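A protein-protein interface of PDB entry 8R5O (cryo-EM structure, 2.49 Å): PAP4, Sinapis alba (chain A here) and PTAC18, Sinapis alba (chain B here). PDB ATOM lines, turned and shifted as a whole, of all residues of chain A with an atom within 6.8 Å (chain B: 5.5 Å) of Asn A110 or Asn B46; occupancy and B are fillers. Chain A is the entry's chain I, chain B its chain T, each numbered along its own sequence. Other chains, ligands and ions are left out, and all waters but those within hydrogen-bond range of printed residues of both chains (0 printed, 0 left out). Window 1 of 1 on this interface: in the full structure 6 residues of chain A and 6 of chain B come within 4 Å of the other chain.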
ATOM      1  N   ARG A  95     -19.250  -6.882 -33.821  1.00  0.00           N
ATOM      2  CA  ARG A  95     -20.173  -7.997 -33.622  1.00  0.00           C
ATOM      3  C   ARG A  95     -21.623  -7.559 -33.789  1.00  0.00           C
ATOM      4  O   ARG A  95     -22.419  -8.265 -34.419  1.00  0.00           O
ATOM      5  CB  ARG A  95     -19.963  -8.621 -32.245  1.00  0.00           C
ATOM      6  CG  ARG A  95     -20.940  -9.740 -31.939  1.00  0.00           C
ATOM      7  CD  ARG A  95     -21.267  -9.796 -30.460  1.00  0.00           C
ATOM      8  NE  ARG A  95     -22.682 -10.065 -30.234  1.00  0.00           N
ATOM      9  CZ  ARG A  95     -23.268 -10.046 -29.045  1.00  0.00           C
ATOM     10  NH1 ARG A  95     -22.587  -9.783 -27.942  1.00  0.00           N
ATOM     11  NH2 ARG A  95     -24.572 -10.294 -28.960  1.00  0.00           N
ATOM     12  N   ILE A 105     -32.104  -6.374 -32.871  1.00  0.00           N
ATOM     13  CA  ILE A 105     -33.078  -6.008 -31.846  1.00  0.00           C
ATOM     14  C   ILE A 105     -33.190  -7.104 -30.796  1.00  0.00           C
ATOM     15  O   ILE A 105     -33.212  -6.830 -29.591  1.00  0.00           O
ATOM     16  CB  ILE A 105     -34.440  -5.703 -32.496  1.00  0.00           C
ATOM     17  CG1 ILE A 105     -34.336  -4.456 -33.370  1.00  0.00           C
ATOM     18  CG2 ILE A 105     -35.516  -5.529 -31.436  1.00  0.00           C
ATOM     19  CD1 ILE A 105     -35.600  -4.142 -34.106  1.00  0.00           C
ATOM     20  N   LYS A 106     -33.266  -8.361 -31.235  1.00  0.00           N
ATOM     21  CA  LYS A 106     -33.369  -9.470 -30.293  1.00  0.00           C
ATOM     22  C   LYS A 106     -32.092  -9.630 -29.480  1.00  0.00           C
ATOM     23  O   LYS A 106     -32.147  -9.925 -28.280  1.00  0.00           O
ATOM     24  CB  LYS A 106     -33.704 -10.758 -31.045  1.00  0.00           C
ATOM     25  CG  LYS A 106     -35.072 -10.729 -31.704  1.00  0.00           C
ATOM     26  CD  LYS A 106     -35.130 -11.607 -32.944  1.00  0.00           C
ATOM     27  CE  LYS A 106     -36.443 -11.407 -33.685  1.00  0.00           C
ATOM     28  NZ  LYS A 106     -36.464 -12.103 -35.000  1.00  0.00           N
ATOM     29  N   ALA A 107     -30.932  -9.444 -30.112  1.00  0.00           N
ATOM     30  CA  ALA A 107     -29.668  -9.593 -29.398  1.00  0.00           C
ATOM     31  C   ALA A 107     -29.472  -8.476 -28.380  1.00  0.00           C
ATOM     32  O   ALA A 107     -29.073  -8.730 -27.237  1.00  0.00           O
ATOM     33  CB  ALA A 107     -28.505  -9.628 -30.390  1.00  0.00           C
ATOM     34  N   THR A 108     -29.746  -7.231 -28.774  1.00  0.00           N
ATOM     35  CA  THR A 108     -29.563  -6.109 -27.860  1.00  0.00           C
ATOM     36  C   THR A 108     -30.620  -6.069 -26.767  1.00  0.00           C
ATOM     37  O   THR A 108     -30.389  -5.450 -25.724  1.00  0.00           O
ATOM     38  CB  THR A 108     -29.564  -4.786 -28.626  1.00  0.00           C
ATOM     39  OG1 THR A 108     -30.733  -4.704 -29.447  1.00  0.00           O
ATOM     40  CG2 THR A 108     -28.325  -4.675 -29.499  1.00  0.00           C
ATOM     41  N   TYR A 109     -31.773  -6.709 -26.978  1.00  0.00           N
ATOM     42  CA  TYR A 109     -32.757  -6.809 -25.906  1.00  0.00           C
ATOM     43  C   TYR A 109     -32.216  -7.632 -24.746  1.00  0.00           C
ATOM     44  O   TYR A 109     -32.549  -7.364 -23.586  1.00  0.00           O
ATOM     45  CB  TYR A 109     -34.057  -7.408 -26.437  1.00  0.00           C
ATOM     46  CG  TYR A 109     -35.139  -7.551 -25.392  1.00  0.00           C
ATOM     47  CD1 TYR A 109     -35.768  -6.433 -24.861  1.00  0.00           C
ATOM     48  CD2 TYR A 109     -35.537  -8.802 -24.944  1.00  0.00           C
ATOM     49  CE1 TYR A 109     -36.756  -6.559 -23.909  1.00  0.00           C
ATOM     50  CE2 TYR A 109     -36.526  -8.935 -23.992  1.00  0.00           C
ATOM     51  CZ  TYR A 109     -37.132  -7.811 -23.478  1.00  0.00           C
ATOM     52  OH  TYR A 109     -38.118  -7.936 -22.530  1.00  0.00           O
ATOM     53  N   ASN A 110     -31.385  -8.634 -25.043  1.00  0.00           N
ATOM     54  CA  ASN A 110     -30.620  -9.371 -24.035  1.00  0.00           C
ATOM     55  C   ASN A 110     -31.531 -10.019 -22.993  1.00  0.00           C
ATOM     56  O   ASN A 110     -31.227 -10.030 -21.798  1.00  0.00           O
ATOM     57  CB  ASN A 110     -29.583  -8.462 -23.370  1.00  0.00           C
ATOM     58  CG  ASN A 110     -28.495  -9.239 -22.660  1.00  0.00           C
ATOM     59  OD1 ASN A 110     -28.148 -10.349 -23.057  1.00  0.00           O
ATOM     60  ND2 ASN A 110     -27.952  -8.657 -21.598  1.00  0.00           N
ATOM     61  N   ASN A 111     -32.660 -10.558 -23.454  1.00  0.00           N
ATOM     62  CA  ASN A 111     -33.573 -11.337 -22.616  1.00  0.00           C
ATOM     63  C   ASN A 111     -34.045 -10.547 -21.395  1.00  0.00           C
ATOM     64  O   ASN A 111     -34.161 -11.084 -20.293  1.00  0.00           O
ATOM     65  CB  ASN A 111     -32.932 -12.662 -22.192  1.00  0.00           C
ATOM     66  CG  ASN A 111     -33.952 -13.686 -21.740  1.00  0.00           C
ATOM     67  OD1 ASN A 111     -35.076 -13.723 -22.240  1.00  0.00           O
ATOM     68  ND2 ASN A 111     -33.566 -14.525 -20.785  1.00  0.00           N
ATOM     69  N   GLY A 112     -34.312  -9.258 -21.586  1.00  0.00           N
ATOM     70  CA  GLY A 112     -34.860  -8.428 -20.534  1.00  0.00           C
ATOM     71  C   GLY A 112     -33.875  -7.537 -19.809  1.00  0.00           C
ATOM     72  O   GLY A 112     -34.275  -6.851 -18.862  1.00  0.00           O
ATOM     73  N   ASN A 113     -32.609  -7.520 -20.217  1.00  0.00           N
ATOM     74  CA  ASN A 113     -31.607  -6.606 -19.668  1.00  0.00           C
ATOM     75  C   ASN A 113     -30.942  -5.886 -20.834  1.00  0.00           C
ATOM     76  O   ASN A 113     -29.796  -6.179 -21.193  1.00  0.00           O
ATOM     77  CB  ASN A 113     -30.585  -7.355 -18.813  1.00  0.00           C
ATOM     78  CG  ASN A 113     -29.678  -6.424 -18.036  1.00  0.00           C
ATOM     79  OD1 ASN A 113     -30.003  -5.256 -17.823  1.00  0.00           O
ATOM     80  ND2 ASN A 113     -28.534  -6.937 -17.606  1.00  0.00           N
ATOM     81  N   PRO A 114     -31.640  -4.926 -21.444  1.00  0.00           N
ATOM     82  CA  PRO A 114     -31.215  -4.409 -22.751  1.00  0.00           C
ATOM     83  C   PRO A 114     -29.843  -3.753 -22.721  1.00  0.00           C
ATOM     84  O   PRO A 114     -29.473  -3.075 -21.761  1.00  0.00           O
ATOM     85  CB  PRO A 114     -32.309  -3.395 -23.100  1.00  0.00           C
ATOM     86  CG  PRO A 114     -33.487  -3.809 -22.288  1.00  0.00           C
ATOM     87  CD  PRO A 114     -32.918  -4.338 -21.011  1.00  0.00           C
ATOM     88  N   LEU A 115     -29.093  -3.963 -23.799  1.00  0.00           N
ATOM     89  CA  LEU A 115     -27.814  -3.315 -24.027  1.00  0.00           C
ATOM     90  C   LEU A 115     -28.030  -1.863 -24.444  1.00  0.00           C
ATOM     91  O   LEU A 115     -29.135  -1.481 -24.832  1.00  0.00           O
ATOM     92  CB  LEU A 115     -27.036  -4.078 -25.096  1.00  0.00           C
ATOM     93  CG  LEU A 115     -26.750  -5.551 -24.794  1.00  0.00           C
ATOM     94  CD1 LEU A 115     -25.896  -6.172 -25.886  1.00  0.00           C
ATOM     95  CD2 LEU A 115     -26.085  -5.706 -23.435  1.00  0.00           C
ATOM     96  N   PHE A 118     -29.968  -1.037 -27.712  1.00  0.00           N
ATOM     97  CA  PHE A 118     -31.318  -1.538 -27.955  1.00  0.00           C
ATOM     98  C   PHE A 118     -32.298  -0.413 -28.264  1.00  0.00           C
ATOM     99  O   PHE A 118     -33.126  -0.543 -29.171  1.00  0.00           O
ATOM    100  CB  PHE A 118     -31.814  -2.349 -26.758  1.00  0.00           C
ATOM    101  CG  PHE A 118     -33.261  -2.738 -26.859  1.00  0.00           C
ATOM    102  CD1 PHE A 118     -33.657  -3.768 -27.694  1.00  0.00           C
ATOM    103  CD2 PHE A 118     -34.229  -2.064 -26.132  1.00  0.00           C
ATOM    104  CE1 PHE A 118     -34.986  -4.122 -27.799  1.00  0.00           C
ATOM    105  CE2 PHE A 118     -35.560  -2.416 -26.232  1.00  0.00           C
ATOM    106  CZ  PHE A 118     -35.939  -3.446 -27.066  1.00  0.00           C
ATOM    107  N   LEU B  41     -15.375 -16.984 -22.351  1.00  0.00           N
ATOM    108  CA  LEU B  41     -16.376 -16.807 -21.304  1.00  0.00           C
ATOM    109  C   LEU B  41     -16.910 -15.379 -21.271  1.00  0.00           C
ATOM    110  O   LEU B  41     -18.097 -15.162 -21.006  1.00  0.00           O
ATOM    111  CB  LEU B  41     -15.792 -17.188 -19.945  1.00  0.00           C
ATOM    112  CG  LEU B  41     -15.573 -18.670 -19.645  1.00  0.00           C
ATOM    113  CD1 LEU B  41     -15.031 -18.840 -18.236  1.00  0.00           C
ATOM    114  CD2 LEU B  41     -16.862 -19.450 -19.821  1.00  0.00           C
ATOM    115  N   GLU B  42     -16.047 -14.391 -21.527  1.00  0.00           N
ATOM    116  CA  GLU B  42     -16.495 -13.003 -21.530  1.00  0.00           C
ATOM    117  C   GLU B  42     -17.558 -12.766 -22.595  1.00  0.00           C
ATOM    118  O   GLU B  42     -18.529 -12.039 -22.364  1.00  0.00           O
ATOM    119  CB  GLU B  42     -15.312 -12.060 -21.746  1.00  0.00           C
ATOM    120  CG  GLU B  42     -14.504 -11.756 -20.498  1.00  0.00           C
ATOM    121  CD  GLU B  42     -13.168 -12.467 -20.478  1.00  0.00           C
ATOM    122  OE1 GLU B  42     -13.127 -13.672 -20.797  1.00  0.00           O
ATOM    123  OE2 GLU B  42     -12.153 -11.814 -20.151  1.00  0.00           O
ATOM    124  N   GLU B  43     -17.382 -13.365 -23.774  1.00  0.00           N
ATOM    125  CA  GLU B  43     -18.386 -13.235 -24.824  1.00  0.00           C
ATOM    126  C   GLU B  43     -19.677 -13.951 -24.446  1.00  0.00           C
ATOM    127  O   GLU B  43     -20.772 -13.414 -24.645  1.00  0.00           O
ATOM    128  CB  GLU B  43     -17.835 -13.781 -26.141  1.00  0.00           C
ATOM    129  CG  GLU B  43     -18.557 -13.273 -27.378  1.00  0.00           C
ATOM    130  CD  GLU B  43     -18.027 -11.932 -27.847  1.00  0.00           C
ATOM    131  OE1 GLU B  43     -16.801 -11.712 -27.759  1.00  0.00           O
ATOM    132  OE2 GLU B  43     -18.835 -11.097 -28.303  1.00  0.00           O
ATOM    133  N   LEU B  44     -19.568 -15.165 -23.900  1.00  0.00           N
ATOM    134  CA  LEU B  44     -20.754 -15.946 -23.566  1.00  0.00           C
ATOM    135  C   LEU B  44     -21.581 -15.278 -22.473  1.00  0.00           C
ATOM    136  O   LEU B  44     -22.812 -15.219 -22.566  1.00  0.00           O
ATOM    137  CB  LEU B  44     -20.352 -17.353 -23.130  1.00  0.00           C
ATOM    138  CG  LEU B  44     -19.837 -18.314 -24.199  1.00  0.00           C
ATOM    139  CD1 LEU B  44     -19.314 -19.586 -23.558  1.00  0.00           C
ATOM    140  CD2 LEU B  44     -20.939 -18.630 -25.193  1.00  0.00           C
ATOM    141  N   TYR B  45     -20.927 -14.770 -21.432  1.00  0.00           N
ATOM    142  CA  TYR B  45     -21.615 -14.256 -20.258  1.00  0.00           C
ATOM    143  C   TYR B  45     -21.808 -12.747 -20.279  1.00  0.00           C
ATOM    144  O   TYR B  45     -22.317 -12.193 -19.301  1.00  0.00           O
ATOM    145  CB  TYR B  45     -20.865 -14.672 -18.990  1.00  0.00           C
ATOM    146  CG  TYR B  45     -21.046 -16.130 -18.651  1.00  0.00           C
ATOM    147  CD1 TYR B  45     -22.082 -16.547 -17.830  1.00  0.00           C
ATOM    148  CD2 TYR B  45     -20.191 -17.096 -19.167  1.00  0.00           C
ATOM    149  CE1 TYR B  45     -22.258 -17.879 -17.523  1.00  0.00           C
ATOM    150  CE2 TYR B  45     -20.361 -18.431 -18.865  1.00  0.00           C
ATOM    151  CZ  TYR B  45     -21.396 -18.816 -18.043  1.00  0.00           C
ATOM    152  OH  TYR B  45     -21.570 -20.146 -17.737  1.00  0.00           O
ATOM    153  N   ASN B  46     -21.421 -12.076 -21.366  1.00  0.00           N
ATOM    154  CA  ASN B  46     -21.623 -10.635 -21.522  1.00  0.00           C
ATOM    155  C   ASN B  46     -20.953  -9.856 -20.388  1.00  0.00           C
ATOM    156  O   ASN B  46     -21.555  -8.994 -19.748  1.00  0.00           O
ATOM    157  CB  ASN B  46     -23.115 -10.300 -21.619  1.00  0.00           C
ATOM    158  CG  ASN B  46     -23.368  -8.860 -22.020  1.00  0.00           C
ATOM    159  OD1 ASN B  46     -22.607  -8.271 -22.788  1.00  0.00           O
ATOM    160  ND2 ASN B  46     -24.439  -8.280 -21.488  1.00  0.00           N
ATOM    161  N   VAL B  47     -19.693 -10.183 -20.131  1.00  0.00           N
ATOM    162  CA  VAL B  47     -18.882  -9.486 -19.141  1.00  0.00           C
ATOM    163  C   VAL B  47     -18.043  -8.468 -19.903  1.00  0.00           C
ATOM    164  O   VAL B  47     -17.030  -8.812 -20.515  1.00  0.00           O
ATOM    165  CB  VAL B  47     -18.013 -10.453 -18.332  1.00  0.00           C
ATOM    166  CG1 VAL B  47     -17.139  -9.685 -17.354  1.00  0.00           C
ATOM    167  CG2 VAL B  47     -18.883 -11.455 -17.597  1.00  0.00           C
ATOM    168  N   LYS B  48     -18.470  -7.209 -19.870  1.00  0.00           N
ATOM    169  CA  LYS B  48     -17.767  -6.147 -20.575  1.00  0.00           C
ATOM    170  C   LYS B  48     -16.518  -5.743 -19.801  1.00  0.00           C
ATOM    171  O   LYS B  48     -16.590  -5.425 -18.611  1.00  0.00           O
ATOM    172  CB  LYS B  48     -18.688  -4.942 -20.771  1.00  0.00           C
ATOM    173  CG  LYS B  48     -18.064  -3.794 -21.540  1.00  0.00           C
ATOM    174  CD  LYS B  48     -19.057  -2.657 -21.728  1.00  0.00           C
ATOM    175  CE  LYS B  48     -18.437  -1.499 -22.491  1.00  0.00           C
ATOM    176  NZ  LYS B  48     -19.400  -0.377 -22.678  1.00  0.00           N
ATOM    177  N   ARG B 113     -17.563  -4.855 -15.868  1.00  0.00           N
ATOM    178  CA  ARG B 113     -18.997  -4.704 -15.648  1.00  0.00           C
ATOM    179  C   ARG B 113     -19.610  -6.093 -15.533  1.00  0.00           C
ATOM    180  O   ARG B 113     -19.775  -6.790 -16.538  1.00  0.00           O
ATOM    181  CB  ARG B 113     -19.653  -3.909 -16.776  1.00  0.00           C
ATOM    182  CG  ARG B 113     -21.105  -3.558 -16.500  1.00  0.00           C
ATOM    183  CD  ARG B 113     -21.755  -2.875 -17.687  1.00  0.00           C
ATOM    184  NE  ARG B 113     -23.106  -2.424 -17.371  1.00  0.00           N
ATOM    185  CZ  ARG B 113     -23.407  -1.205 -16.945  1.00  0.00           C
ATOM    186  NH1 ARG B 113     -22.478  -0.276 -16.798  1.00  0.00           N
ATOM    187  NH2 ARG B 113     -24.672  -0.911 -16.664  1.00  0.00           N
ATOM    188  N   PRO B 115     -22.649  -8.430 -15.299  1.00  0.00           N
ATOM    189  CA  PRO B 115     -24.048  -8.255 -15.695  1.00  0.00           C
ATOM    190  C   PRO B 115     -25.022  -8.743 -14.630  1.00  0.00           C
ATOM    191  O   PRO B 115     -24.698  -9.554 -13.764  1.00  0.00           O
ATOM    192  CB  PRO B 115     -24.160  -9.105 -16.965  1.00  0.00           C
ATOM    193  CG  PRO B 115     -23.141 -10.170 -16.775  1.00  0.00           C
ATOM    194  CD  PRO B 115     -22.001  -9.534 -16.029  1.00  0.00           C
ATOM    195  N   TRP B 117     -27.976 -10.887 -13.112  1.00  0.00           N
ATOM    196  CA  TRP B 117     -28.345 -12.307 -13.128  1.00  0.00           C
ATOM    197  C   TRP B 117     -27.147 -13.226 -13.331  1.00  0.00           C
ATOM    198  O   TRP B 117     -27.341 -14.413 -13.619  1.00  0.00           O
ATOM    199  CB  TRP B 117     -29.400 -12.631 -14.191  1.00  0.00           C
ATOM    200  CG  TRP B 117     -30.684 -11.896 -14.003  1.00  0.00           C
ATOM    201  CD1 TRP B 117     -31.306 -11.627 -12.823  1.00  0.00           C
ATOM    202  CD2 TRP B 117     -31.498 -11.316 -15.029  1.00  0.00           C
ATOM    203  NE1 TRP B 117     -32.465 -10.925 -13.049  1.00  0.00           N
ATOM    204  CE2 TRP B 117     -32.603 -10.720 -14.395  1.00  0.00           C
ATOM    205  CE3 TRP B 117     -31.399 -11.247 -16.419  1.00  0.00           C
ATOM    206  CZ2 TRP B 117     -33.604 -10.063 -15.104  1.00  0.00           C
ATOM    207  CZ3 TRP B 117     -32.393 -10.595 -17.123  1.00  0.00           C
ATOM    208  CH2 TRP B 117     -33.481 -10.011 -16.465  1.00  0.00           C
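O of Thr A108 lies within hydrogen-bond range of N of Leu A115, at 2.8 Å. O of Asn A113 is in hydrogen-bond range of ND2 of Asn A110 (3.1 Å).
Hydrophobic or aromatic side chains of chain A that line the printed part of chain B: Leu A115. Hydrophobic or aromatic side chains of chain B within 4 Å of the printed part of chain A: Trp B117. Among the printed residues, Asp or Glu carboxylates within 4 Å of a Lys or Arg side-chain nitrogen of the other chain: Arg A95 with Glu B43.
Of the printed residues of chain A, Asn B46 touches Asn A110 (3.5 Å) and Leu A115 (3.6 Å). Of the printed residues of chain B, Asn A111 touches Trp B117. Of the printed residues of chain B, Arg A95 touches Glu B43 (3.5 Å). Of the printed residues of chain A, Trp B117 touches Asn A111 (3.7 Å). Of the printed residues of chain B, Leu A115 touches Asn B46 (3.6 Å). Printed residues of chain A within 4 Å of Glu B43: Arg A95. Pro A114 touches none of the printed residues of chain B. Lys B48 touches none of the printed residues of chain A. The nearest printed residue of chain B that does not touch Asn A111 is Asn B46 (8.8 Å).
Asn B46 touches Asn A110. CZ3 of Trp B117 touches O of Asn A111, 3.7 Å away. Asn B46 touches Leu A115.
The side-chain carboxylate of Glu B43 is in salt-bridge range of the guanidinium group of Arg A95 (3.99 Å).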
